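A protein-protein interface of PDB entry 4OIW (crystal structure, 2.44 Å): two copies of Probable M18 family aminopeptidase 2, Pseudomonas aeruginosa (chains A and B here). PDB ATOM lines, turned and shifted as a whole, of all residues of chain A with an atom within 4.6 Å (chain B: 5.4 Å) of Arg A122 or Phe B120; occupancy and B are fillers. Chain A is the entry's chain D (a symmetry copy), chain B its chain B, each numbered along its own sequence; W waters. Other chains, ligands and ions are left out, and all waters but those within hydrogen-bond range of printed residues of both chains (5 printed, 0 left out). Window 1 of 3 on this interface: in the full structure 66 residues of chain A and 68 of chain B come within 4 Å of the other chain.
Of chain B, only Phe B120, Asp B121 and Arg B122 come within 4 Å of Arg A122.
Of chain A, only Arg A122 (3.3 Å) and Tyr A318 (3.5 Å) come within 4 Å of Phe B120.
Of the printed residues of chain B, Arg A406 touches Asp B121 (3.4 Å).
Of the printed residues of chain B, Pro A118 touches Asn B154.
Of the printed residues of chain B, Phe A120 touches Arg B122.
Printed residues of chain A within 4 Å of Arg B406: Asp A121 (3.4 Å) and Asp A123 (2.7 Å).
Of the printed residues of chain A, Glu B174 touches Tyr A318 (2.7 Å).
Phe B116 touches none of the printed residues of chain A.
Leu A124 touches none of the printed residues of chain B.
The nearest residue of chain B that does not touch Arg A122 is Arg B406 (4.9 Å).
The nearest printed residue of chain A that does not touch Phe B120 is Pro A118 (5.7 Å).
Phe A120 touches Arg B122, and with the chains exchanged Arg A122 touches Phe B120.
Asp A121 touches Arg B122, and with the chains exchanged Arg A122 touches Asp B121.
Asp A121 touches Arg B406, and with the chains exchanged Arg A406 touches Asp B121.
Arg B122 touches its own counterpart, Arg A122.
Positions printed for both chains: 118, 119, 120, 121, 122 and 406.
Of the 11 pairs that touch across the chains among the printed residues, 7 have their exchanged pair printed and touching as well.
Water W5 lies within hydrogen-bond range of O of Phe B120 (2.7 Å), NH2 of Arg A122 (3.0 Å) and O of Ala B117 (3.3 Å).
Water W2 bridges the side-chain amide oxygen of Asn B154 and the side-chain hydroxyl of Tyr A318.
Water W1 lies within hydrogen-bond range of O of Arg B406 (2.8 Å) and OD1 of Asp A121 (2.8 Å).
Water W3 lies within hydrogen-bond range of the backbone carbonyl oxygen (O) of Arg A406 (2.8 Å) and the side-chain carboxylate (OD1) of Asp B121 (3.0 Å).
Water W4 lies within hydrogen-bond range of O of Phe A120 and NH2 of Arg B122.
Among the printed residues, merely in contact across the chains: Arg A406 with Asp B121, Asp A121 with Arg B406, Pro A118 with Asn B154, Tyr A318 with Phe B120 and Arg A122 with Arg B122.
OE1 of Glu B174 is in hydrogen-bond range of OH of Tyr A318 (2.7 Å).
The side-chain carboxylate of Asp A123 lies within salt-bridge range of the guanidinium group of Arg B406, 2.7 Å away.
The guanidinium group of Arg B122 is in hydrogen-bond range of the backbone carbonyl oxygen of Asp A121, at 2.9 Å.
The guanidinium group of Arg B122 is in hydrogen-bond range of the backbone carbonyl oxygen of Phe A120.
O of Phe B120 sits at hydrogen-bond distance from NH2 of Arg A122, at 3.3 Å.
The backbone carbonyl oxygen (O) of Asp B121 is in hydrogen-bond range of the guanidinium group (NH2) of Arg A122 (2.9 Å).
Hydrophobic or aromatic side chains of chain A within 4 Å of the printed part of chain B: Pro A118 and Tyr A318.
Of the 14 printed residues of chain B, 6 touch a printed residue of chain A.
Hydrophobic or aromatic side chains of chain B that line the printed part of chain A: Phe B120.
Among the printed residues, 11 pairs touch across the chains.
N of Asp B121 is in hydrogen-bond range of O of Ile B152.
The guanidinium group (NE) of Arg A122 lies within hydrogen-bond range of the backbone carbonyl oxygen (O) of Pro A118 (2.9 Å).
The side-chain carboxylate (OD2) of Asp B121 is in hydrogen-bond range of the side-chain amide nitrogen (ND2) of Asn B154 (2.6 Å).
NE of Arg B122 is in hydrogen-bond range of O of Pro B118, at 2.8 Å.
NH1 of Arg A406 is in hydrogen-bond range of O of Gln A220.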
ATOM      1  N   PRO A 118      -8.205   5.379 -20.009  1.00  0.00           N
ATOM      2  CA  PRO A 118      -6.769   5.654 -19.930  1.00  0.00           C
ATOM      3  C   PRO A 118      -6.163   5.958 -18.557  1.00  0.00           C
ATOM      4  O   PRO A 118      -4.965   5.811 -18.411  1.00  0.00           O
ATOM      5  CB  PRO A 118      -6.615   6.881 -20.824  1.00  0.00           C
ATOM      6  CG  PRO A 118      -7.718   6.759 -21.778  1.00  0.00           C
ATOM      7  CD  PRO A 118      -8.860   6.332 -20.894  1.00  0.00           C
ATOM      8  N   TRP A 119      -6.951   6.414 -17.581  1.00  0.00           N
ATOM      9  CA  TRP A 119      -6.411   6.720 -16.249  1.00  0.00           C
ATOM     10  C   TRP A 119      -6.000   5.449 -15.461  1.00  0.00           C
ATOM     11  O   TRP A 119      -5.230   5.523 -14.497  1.00  0.00           O
ATOM     12  CB  TRP A 119      -7.387   7.608 -15.464  1.00  0.00           C
ATOM     13  CG  TRP A 119      -7.300   9.018 -15.918  1.00  0.00           C
ATOM     14  CD1 TRP A 119      -7.880   9.572 -17.055  1.00  0.00           C
ATOM     15  CD2 TRP A 119      -6.565  10.070 -15.294  1.00  0.00           C
ATOM     16  NE1 TRP A 119      -7.538  10.887 -17.156  1.00  0.00           N
ATOM     17  CE2 TRP A 119      -6.709  11.216 -16.105  1.00  0.00           C
ATOM     18  CE3 TRP A 119      -5.796  10.162 -14.128  1.00  0.00           C
ATOM     19  CZ2 TRP A 119      -6.119  12.434 -15.774  1.00  0.00           C
ATOM     20  CZ3 TRP A 119      -5.197  11.369 -13.820  1.00  0.00           C
ATOM     21  CH2 TRP A 119      -5.374  12.485 -14.628  1.00  0.00           C
ATOM     22  N   PHE A 120      -6.482   4.284 -15.896  1.00  0.00           N
ATOM     23  CA  PHE A 120      -6.147   3.039 -15.242  1.00  0.00           C
ATOM     24  C   PHE A 120      -4.733   2.604 -15.556  1.00  0.00           C
ATOM     25  O   PHE A 120      -4.252   2.808 -16.669  1.00  0.00           O
ATOM     26  CB  PHE A 120      -7.065   1.924 -15.674  1.00  0.00           C
ATOM     27  CG  PHE A 120      -8.452   2.030 -15.135  1.00  0.00           C
ATOM     28  CD1 PHE A 120      -9.337   2.939 -15.639  1.00  0.00           C
ATOM     29  CD2 PHE A 120      -8.887   1.161 -14.168  1.00  0.00           C
ATOM     30  CE1 PHE A 120     -10.649   2.992 -15.180  1.00  0.00           C
ATOM     31  CE2 PHE A 120     -10.183   1.218 -13.687  1.00  0.00           C
ATOM     32  CZ  PHE A 120     -11.070   2.136 -14.198  1.00  0.00           C
ATOM     33  N   ASP A 121      -4.084   1.982 -14.572  1.00  0.00           N
ATOM     34  CA  ASP A 121      -2.792   1.319 -14.806  1.00  0.00           C
ATOM     35  C   ASP A 121      -1.735   2.317 -15.267  1.00  0.00           C
ATOM     36  O   ASP A 121      -0.967   2.053 -16.175  1.00  0.00           O
ATOM     37  CB  ASP A 121      -2.951   0.170 -15.813  1.00  0.00           C
ATOM     38  CG  ASP A 121      -3.919  -0.931 -15.334  1.00  0.00           C
ATOM     39  OD1 ASP A 121      -4.199  -1.022 -14.077  1.00  0.00           O
ATOM     40  OD2 ASP A 121      -4.384  -1.715 -16.229  1.00  0.00           O
ATOM     41  N   ARG A 122      -1.694   3.441 -14.578  1.00  0.00           N
ATOM     42  CA  ARG A 122      -0.737   4.528 -14.778  1.00  0.00           C
ATOM     43  C   ARG A 122      -0.179   4.893 -13.433  1.00  0.00           C
ATOM     44  O   ARG A 122      -0.895   4.870 -12.412  1.00  0.00           O
ATOM     45  CB  ARG A 122      -1.456   5.811 -15.262  1.00  0.00           C
ATOM     46  CG  ARG A 122      -2.197   5.646 -16.569  1.00  0.00           C
ATOM     47  CD  ARG A 122      -1.289   5.736 -17.776  1.00  0.00           C
ATOM     48  NE  ARG A 122      -2.092   5.555 -18.986  1.00  0.00           N
ATOM     49  CZ  ARG A 122      -1.656   5.685 -20.242  1.00  0.00           C
ATOM     50  NH1 ARG A 122      -0.396   6.027 -20.500  1.00  0.00           N
ATOM     51  NH2 ARG A 122      -2.491   5.457 -21.256  1.00  0.00           N
ATOM     52  N   ASP A 123       1.067   5.312 -13.451  1.00  0.00           N
ATOM     53  CA  ASP A 123       1.765   5.693 -12.264  1.00  0.00           C
ATOM     54  C   ASP A 123       1.475   7.163 -12.013  1.00  0.00           C
ATOM     55  O   ASP A 123       2.028   8.051 -12.703  1.00  0.00           O
ATOM     56  CB  ASP A 123       3.262   5.487 -12.482  1.00  0.00           C
ATOM     57  CG  ASP A 123       3.647   4.024 -12.780  1.00  0.00           C
ATOM     58  OD1 ASP A 123       2.807   3.106 -12.881  1.00  0.00           O
ATOM     59  OD2 ASP A 123       4.851   3.772 -12.856  1.00  0.00           O
ATOM     60  N   LEU A 124       0.644   7.415 -11.007  1.00  0.00           N
ATOM     61  CA  LEU A 124       0.116   8.740 -10.722  1.00  0.00           C
ATOM     62  C   LEU A 124       0.731   9.406  -9.476  1.00  0.00           C
ATOM     63  O   LEU A 124       1.077   8.752  -8.490  1.00  0.00           O
ATOM     64  CB  LEU A 124      -1.377   8.640 -10.504  1.00  0.00           C
ATOM     65  CG  LEU A 124      -2.214   8.056 -11.640  1.00  0.00           C
ATOM     66  CD1 LEU A 124      -3.675   7.974 -11.212  1.00  0.00           C
ATOM     67  CD2 LEU A 124      -2.118   8.888 -12.891  1.00  0.00           C
ATOM     68  N   ALA A 150       0.124   6.839  -6.412  1.00  0.00           N
ATOM     69  CA  ALA A 150      -1.250   6.348  -6.615  1.00  0.00           C
ATOM     70  C   ALA A 150      -1.382   5.565  -7.887  1.00  0.00           C
ATOM     71  O   ALA A 150      -0.655   5.783  -8.845  1.00  0.00           O
ATOM     72  CB  ALA A 150      -2.237   7.493  -6.645  1.00  0.00           C
ATOM     73  N   VAL A 151      -2.331   4.642  -7.890  1.00  0.00           N
ATOM     74  CA  VAL A 151      -2.638   3.843  -9.095  1.00  0.00           C
ATOM     75  C   VAL A 151      -4.097   3.446  -9.029  1.00  0.00           C
ATOM     76  O   VAL A 151      -4.639   3.188  -7.948  1.00  0.00           O
ATOM     77  CB  VAL A 151      -1.757   2.602  -9.171  1.00  0.00           C
ATOM     78  CG1 VAL A 151      -1.816   1.844  -7.833  1.00  0.00           C
ATOM     79  CG2 VAL A 151      -2.142   1.692 -10.347  1.00  0.00           C
ATOM     80  N   ASP A 218      -0.247  11.900 -14.368  1.00  0.00           N
ATOM     81  CA  ASP A 218       0.724  10.943 -14.812  1.00  0.00           C
ATOM     82  C   ASP A 218       2.182  11.359 -14.603  1.00  0.00           C
ATOM     83  O   ASP A 218       2.601  12.423 -15.060  1.00  0.00           O
ATOM     84  CB  ASP A 218       0.520  10.720 -16.337  1.00  0.00           C
ATOM     85  CG  ASP A 218       1.140   9.404 -16.811  1.00  0.00           C
ATOM     86  OD1 ASP A 218       1.892   8.875 -15.981  1.00  0.00           O
ATOM     87  OD2 ASP A 218       0.853   8.879 -17.935  1.00  0.00           O
ATOM     88  N   GLN A 220       4.639   9.873 -16.016  1.00  0.00           N
ATOM     89  CA  GLN A 220       5.371   9.688 -17.268  1.00  0.00           C
ATOM     90  C   GLN A 220       5.419  10.978 -18.052  1.00  0.00           C
ATOM     91  O   GLN A 220       4.421  11.487 -18.562  1.00  0.00           O
ATOM     92  CB  GLN A 220       4.780   8.581 -18.132  1.00  0.00           C
ATOM     93  CG  GLN A 220       5.558   8.353 -19.435  1.00  0.00           C
ATOM     94  CD  GLN A 220       4.914   7.266 -20.291  1.00  0.00           C
ATOM     95  OE1 GLN A 220       3.709   7.253 -20.444  1.00  0.00           O
ATOM     96  NE2 GLN A 220       5.704   6.345 -20.827  1.00  0.00           N
ATOM     97  N   TYR A 318     -10.005   5.423 -37.038  1.00  0.00           N
ATOM     98  CA  TYR A 318     -11.399   5.891 -36.938  1.00  0.00           C
ATOM     99  C   TYR A 318     -11.738   7.008 -37.914  1.00  0.00           C
ATOM    100  O   TYR A 318     -12.337   8.028 -37.542  1.00  0.00           O
ATOM    101  CB  TYR A 318     -11.708   6.381 -35.512  1.00  0.00           C
ATOM    102  CG  TYR A 318     -11.317   5.485 -34.349  1.00  0.00           C
ATOM    103  CD1 TYR A 318     -10.070   5.596 -33.747  1.00  0.00           C
ATOM    104  CD2 TYR A 318     -12.208   4.586 -33.814  1.00  0.00           C
ATOM    105  CE1 TYR A 318      -9.732   4.815 -32.651  1.00  0.00           C
ATOM    106  CE2 TYR A 318     -11.883   3.809 -32.731  1.00  0.00           C
ATOM    107  CZ  TYR A 318     -10.644   3.920 -32.144  1.00  0.00           C
ATOM    108  OH  TYR A 318     -10.327   3.140 -31.025  1.00  0.00           O
ATOM    109  N   ILE A 405      -5.344  10.660 -20.854  1.00  0.00           N
ATOM    110  CA  ILE A 405      -4.289  10.995 -19.945  1.00  0.00           C
ATOM    111  C   ILE A 405      -3.015  11.193 -20.725  1.00  0.00           C
ATOM    112  O   ILE A 405      -2.042  11.661 -20.178  1.00  0.00           O
ATOM    113  CB  ILE A 405      -4.094   9.870 -18.873  1.00  0.00           C
ATOM    114  CG1 ILE A 405      -3.412  10.469 -17.640  1.00  0.00           C
ATOM    115  CG2 ILE A 405      -3.315   8.678 -19.447  1.00  0.00           C
ATOM    116  CD1 ILE A 405      -3.128   9.472 -16.547  1.00  0.00           C
ATOM    117  N   ARG A 406      -3.008  10.763 -21.987  1.00  0.00           N
ATOM    118  CA  ARG A 406      -1.864  10.898 -22.870  1.00  0.00           C
ATOM    119  C   ARG A 406      -2.342  11.125 -24.315  1.00  0.00           C
ATOM    120  O   ARG A 406      -2.758  10.208 -24.991  1.00  0.00           O
ATOM    121  CB  ARG A 406      -0.942   9.659 -22.763  1.00  0.00           C
ATOM    122  CG  ARG A 406       0.513   9.907 -23.171  1.00  0.00           C
ATOM    123  CD  ARG A 406       1.441   8.737 -22.806  1.00  0.00           C
ATOM    124  NE  ARG A 406       2.861   8.943 -23.120  1.00  0.00           N
ATOM    125  CZ  ARG A 406       3.675   9.743 -22.429  1.00  0.00           C
ATOM    126  NH1 ARG A 406       3.226  10.463 -21.378  1.00  0.00           N
ATOM    127  NH2 ARG A 406       4.947   9.824 -22.777  1.00  0.00           N
ATOM    128  N   PHE B 116      -7.583  -4.951 -23.992  1.00  0.00           N
ATOM    129  CA  PHE B 116      -7.253  -4.085 -25.109  1.00  0.00           C
ATOM    130  C   PHE B 116      -7.064  -2.632 -24.658  1.00  0.00           C
ATOM    131  O   PHE B 116      -6.134  -1.974 -25.072  1.00  0.00           O
ATOM    132  CB  PHE B 116      -8.367  -4.125 -26.183  1.00  0.00           C
ATOM    133  CG  PHE B 116      -8.580  -5.479 -26.865  1.00  0.00           C
ATOM    134  CD1 PHE B 116      -7.672  -6.529 -26.732  1.00  0.00           C
ATOM    135  CD2 PHE B 116      -9.718  -5.678 -27.687  1.00  0.00           C
ATOM    136  CE1 PHE B 116      -7.901  -7.764 -27.370  1.00  0.00           C
ATOM    137  CE2 PHE B 116      -9.918  -6.874 -28.366  1.00  0.00           C
ATOM    138  CZ  PHE B 116      -9.011  -7.930 -28.200  1.00  0.00           C
ATOM    139  N   ALA B 117      -7.940  -2.126 -23.805  1.00  0.00           N
ATOM    140  CA  ALA B 117      -7.942  -0.697 -23.508  1.00  0.00           C
ATOM    141  C   ALA B 117      -6.596  -0.138 -22.999  1.00  0.00           C
ATOM    142  O   ALA B 117      -6.190   0.940 -23.381  1.00  0.00           O
ATOM    143  CB  ALA B 117      -9.058  -0.359 -22.548  1.00  0.00           C
ATOM    144  N   PRO B 118      -5.900  -0.871 -22.143  1.00  0.00           N
ATOM    145  CA  PRO B 118      -4.637  -0.335 -21.641  1.00  0.00           C
ATOM    146  C   PRO B 118      -3.560  -0.157 -22.666  1.00  0.00           C
ATOM    147  O   PRO B 118      -2.636   0.584 -22.401  1.00  0.00           O
ATOM    148  CB  PRO B 118      -4.175  -1.387 -20.637  1.00  0.00           C
ATOM    149  CG  PRO B 118      -5.402  -2.063 -20.187  1.00  0.00           C
ATOM    150  CD  PRO B 118      -6.382  -2.010 -21.342  1.00  0.00           C
ATOM    151  N   TRP B 119      -3.612  -0.858 -23.794  1.00  0.00           N
ATOM    152  CA  TRP B 119      -2.576  -0.682 -24.836  1.00  0.00           C
ATOM    153  C   TRP B 119      -2.689   0.649 -25.557  1.00  0.00           C
ATOM    154  O   TRP B 119      -1.748   1.041 -26.254  1.00  0.00           O
ATOM    155  CB  TRP B 119      -2.560  -1.819 -25.882  1.00  0.00           C
ATOM    156  CG  TRP B 119      -2.001  -3.052 -25.303  1.00  0.00           C
ATOM    157  CD1 TRP B 119      -2.642  -3.892 -24.428  1.00  0.00           C
ATOM    158  CD2 TRP B 119      -0.676  -3.553 -25.438  1.00  0.00           C
ATOM    159  NE1 TRP B 119      -1.792  -4.890 -24.033  1.00  0.00           N
ATOM    160  CE2 TRP B 119      -0.580  -4.702 -24.632  1.00  0.00           C
ATOM    161  CE3 TRP B 119       0.434  -3.150 -26.163  1.00  0.00           C
ATOM    162  CZ2 TRP B 119       0.569  -5.465 -24.555  1.00  0.00           C
ATOM    163  CZ3 TRP B 119       1.584  -3.894 -26.073  1.00  0.00           C
ATOM    164  CH2 TRP B 119       1.650  -5.039 -25.272  1.00  0.00           C
ATOM    165  N   PHE B 120      -3.809   1.341 -25.413  1.00  0.00           N
ATOM    166  CA  PHE B 120      -3.925   2.621 -26.016  1.00  0.00           C
ATOM    167  C   PHE B 120      -3.180   3.695 -25.230  1.00  0.00           C
ATOM    168  O   PHE B 120      -3.131   3.673 -23.985  1.00  0.00           O
ATOM    169  CB  PHE B 120      -5.380   3.050 -26.105  1.00  0.00           C
ATOM    170  CG  PHE B 120      -6.228   2.244 -27.072  1.00  0.00           C
ATOM    171  CD1 PHE B 120      -6.643   0.910 -26.766  1.00  0.00           C
ATOM    172  CD2 PHE B 120      -6.719   2.841 -28.223  1.00  0.00           C
ATOM    173  CE1 PHE B 120      -7.456   0.217 -27.646  1.00  0.00           C
ATOM    174  CE2 PHE B 120      -7.548   2.154 -29.078  1.00  0.00           C
ATOM    175  CZ  PHE B 120      -7.914   0.849 -28.802  1.00  0.00           C
ATOM    176  N   ASP B 121      -2.689   4.678 -25.976  1.00  0.00           N
ATOM    177  CA  ASP B 121      -2.041   5.881 -25.445  1.00  0.00           C
ATOM    178  C   ASP B 121      -0.821   5.535 -24.560  1.00  0.00           C
ATOM    179  O   ASP B 121      -0.655   6.096 -23.419  1.00  0.00           O
ATOM    180  CB  ASP B 121      -3.046   6.793 -24.705  1.00  0.00           C
ATOM    181  CG  ASP B 121      -4.253   7.185 -25.582  1.00  0.00           C
ATOM    182  OD1 ASP B 121      -4.125   7.199 -26.823  1.00  0.00           O
ATOM    183  OD2 ASP B 121      -5.355   7.458 -25.031  1.00  0.00           O
ATOM    184  N   ARG B 122      -0.008   4.622 -25.114  1.00  0.00           N
ATOM    185  CA  ARG B 122       1.244   4.187 -24.537  1.00  0.00           C
ATOM    186  C   ARG B 122       2.379   4.326 -25.547  1.00  0.00           C
ATOM    187  O   ARG B 122       2.204   4.094 -26.779  1.00  0.00           O
ATOM    188  CB  ARG B 122       1.181   2.696 -24.191  1.00  0.00           C
ATOM    189  CG  ARG B 122       0.022   2.308 -23.294  1.00  0.00           C
ATOM    190  CD  ARG B 122       0.347   2.482 -21.821  1.00  0.00           C
ATOM    191  NE  ARG B 122      -0.795   2.187 -20.963  1.00  0.00           N
ATOM    192  CZ  ARG B 122      -0.787   2.245 -19.631  1.00  0.00           C
ATOM    193  NH1 ARG B 122       0.291   2.591 -18.962  1.00  0.00           N
ATOM    194  NH2 ARG B 122      -1.877   1.949 -18.962  1.00  0.00           N
ATOM    195  N   ILE B 152      -0.799   3.502 -30.205  1.00  0.00           N
ATOM    196  CA  ILE B 152      -2.195   3.218 -30.525  1.00  0.00           C
ATOM    197  C   ILE B 152      -3.070   4.281 -29.833  1.00  0.00           C
ATOM    198  O   ILE B 152      -3.512   4.103 -28.675  1.00  0.00           O
ATOM    199  CB  ILE B 152      -2.626   1.838 -30.013  1.00  0.00           C
ATOM    200  CG1 ILE B 152      -1.703   0.723 -30.481  1.00  0.00           C
ATOM    201  CG2 ILE B 152      -4.012   1.469 -30.535  1.00  0.00           C
ATOM    202  CD1 ILE B 152      -1.963  -0.553 -29.704  1.00  0.00           C
ATOM    203  N   PRO B 153      -3.380   5.373 -30.541  1.00  0.00           N
ATOM    204  CA  PRO B 153      -4.044   6.465 -29.882  1.00  0.00           C
ATOM    205  C   PRO B 153      -5.501   6.217 -29.712  1.00  0.00           C
ATOM    206  O   PRO B 153      -6.149   5.722 -30.655  1.00  0.00           O
ATOM    207  CB  PRO B 153      -3.877   7.617 -30.864  1.00  0.00           C
ATOM    208  CG  PRO B 153      -2.791   7.188 -31.781  1.00  0.00           C
ATOM    209  CD  PRO B 153      -3.065   5.721 -31.920  1.00  0.00           C
ATOM    210  N   ASN B 154      -6.058   6.604 -28.564  1.00  0.00           N
ATOM    211  CA  ASN B 154      -7.504   6.672 -28.490  1.00  0.00           C
ATOM    212  C   ASN B 154      -8.083   7.684 -29.488  1.00  0.00           C
ATOM    213  O   ASN B 154      -7.403   8.559 -29.968  1.00  0.00           O
ATOM    214  CB  ASN B 154      -7.964   7.060 -27.100  1.00  0.00           C
ATOM    215  CG  ASN B 154      -8.143   5.855 -26.185  1.00  0.00           C
ATOM    216  OD1 ASN B 154      -8.954   4.976 -26.467  1.00  0.00           O
ATOM    217  ND2 ASN B 154      -7.413   5.832 -25.069  1.00  0.00           N
ATOM    218  N   ILE B 169     -14.221  -2.995 -28.234  1.00  0.00           N
ATOM    219  CA  ILE B 169     -13.054  -2.708 -29.038  1.00  0.00           C
ATOM    220  C   ILE B 169     -12.786  -3.819 -30.071  1.00  0.00           C
ATOM    221  O   ILE B 169     -12.637  -4.998 -29.755  1.00  0.00           O
ATOM    222  CB  ILE B 169     -11.803  -2.464 -28.149  1.00  0.00           C
ATOM    223  CG1 ILE B 169     -11.977  -1.171 -27.310  1.00  0.00           C
ATOM    224  CG2 ILE B 169     -10.527  -2.358 -28.993  1.00  0.00           C
ATOM    225  CD1 ILE B 169     -11.161  -1.174 -26.041  1.00  0.00           C
ATOM    226  N   GLU B 174      -9.010  -1.198 -34.477  1.00  0.00           N
ATOM    227  CA  GLU B 174      -8.558  -0.193 -33.515  1.00  0.00           C
ATOM    228  C   GLU B 174      -7.188  -0.452 -32.899  1.00  0.00           C
ATOM    229  O   GLU B 174      -6.630   0.486 -32.369  1.00  0.00           O
ATOM    230  CB  GLU B 174      -9.580   0.019 -32.397  1.00  0.00           C
ATOM    231  CG  GLU B 174     -10.995   0.246 -32.898  1.00  0.00           C
ATOM    232  CD  GLU B 174     -12.025   0.189 -31.817  1.00  0.00           C
ATOM    233  OE1 GLU B 174     -11.934   0.968 -30.867  1.00  0.00           O
ATOM    234  OE2 GLU B 174     -12.963  -0.607 -31.937  1.00  0.00           O
ATOM    235  N   LEU B 175      -6.627  -1.672 -33.005  1.00  0.00           N
ATOM    236  CA  LEU B 175      -5.301  -1.961 -32.443  1.00  0.00           C
ATOM    237  C   LEU B 175      -4.079  -1.660 -33.291  1.00  0.00           C
ATOM    238  O   LEU B 175      -2.991  -1.563 -32.740  1.00  0.00           O
ATOM    239  CB  LEU B 175      -5.201  -3.418 -31.958  1.00  0.00           C
ATOM    240  CG  LEU B 175      -6.076  -3.568 -30.699  1.00  0.00           C
ATOM    241  CD1 LEU B 175      -5.893  -4.870 -29.938  1.00  0.00           C
ATOM    242  CD2 LEU B 175      -5.834  -2.451 -29.712  1.00  0.00           C
ATOM    243  N   ARG B 406       0.106  -3.039 -17.978  1.00  0.00           N
ATOM    244  CA  ARG B 406       0.806  -2.667 -16.748  1.00  0.00           C
ATOM    245  C   ARG B 406       0.068  -3.195 -15.531  1.00  0.00           C
ATOM    246  O   ARG B 406      -0.955  -2.640 -15.107  1.00  0.00           O
ATOM    247  CB  ARG B 406       0.930  -1.156 -16.624  1.00  0.00           C
ATOM    248  CG  ARG B 406       2.131  -0.703 -15.777  1.00  0.00           C
ATOM    249  CD  ARG B 406       2.337   0.823 -15.904  1.00  0.00           C
ATOM    250  NE  ARG B 406       3.417   1.370 -15.062  1.00  0.00           N
ATOM    251  CZ  ARG B 406       4.721   1.211 -15.318  1.00  0.00           C
ATOM    252  NH1 ARG B 406       5.149   0.479 -16.347  1.00  0.00           N
ATOM    253  NH2 ARG B 406       5.623   1.737 -14.519  1.00  0.00           N
HETATM  254  O   HOH W   1      -1.902  -1.770 -12.640  1.00  0.00           O
HETATM  255  O   HOH W   2     -10.391   4.887 -28.723  1.00  0.00           O
HETATM  256  O   HOH W   3      -1.936   9.108 -27.427  1.00  0.00           O
HETATM  257  O   HOH W   4      -4.778   2.316 -19.407  1.00  0.00           O
HETATM  258  O   HOH W   5      -4.648   3.421 -21.809  1.00  0.00           O
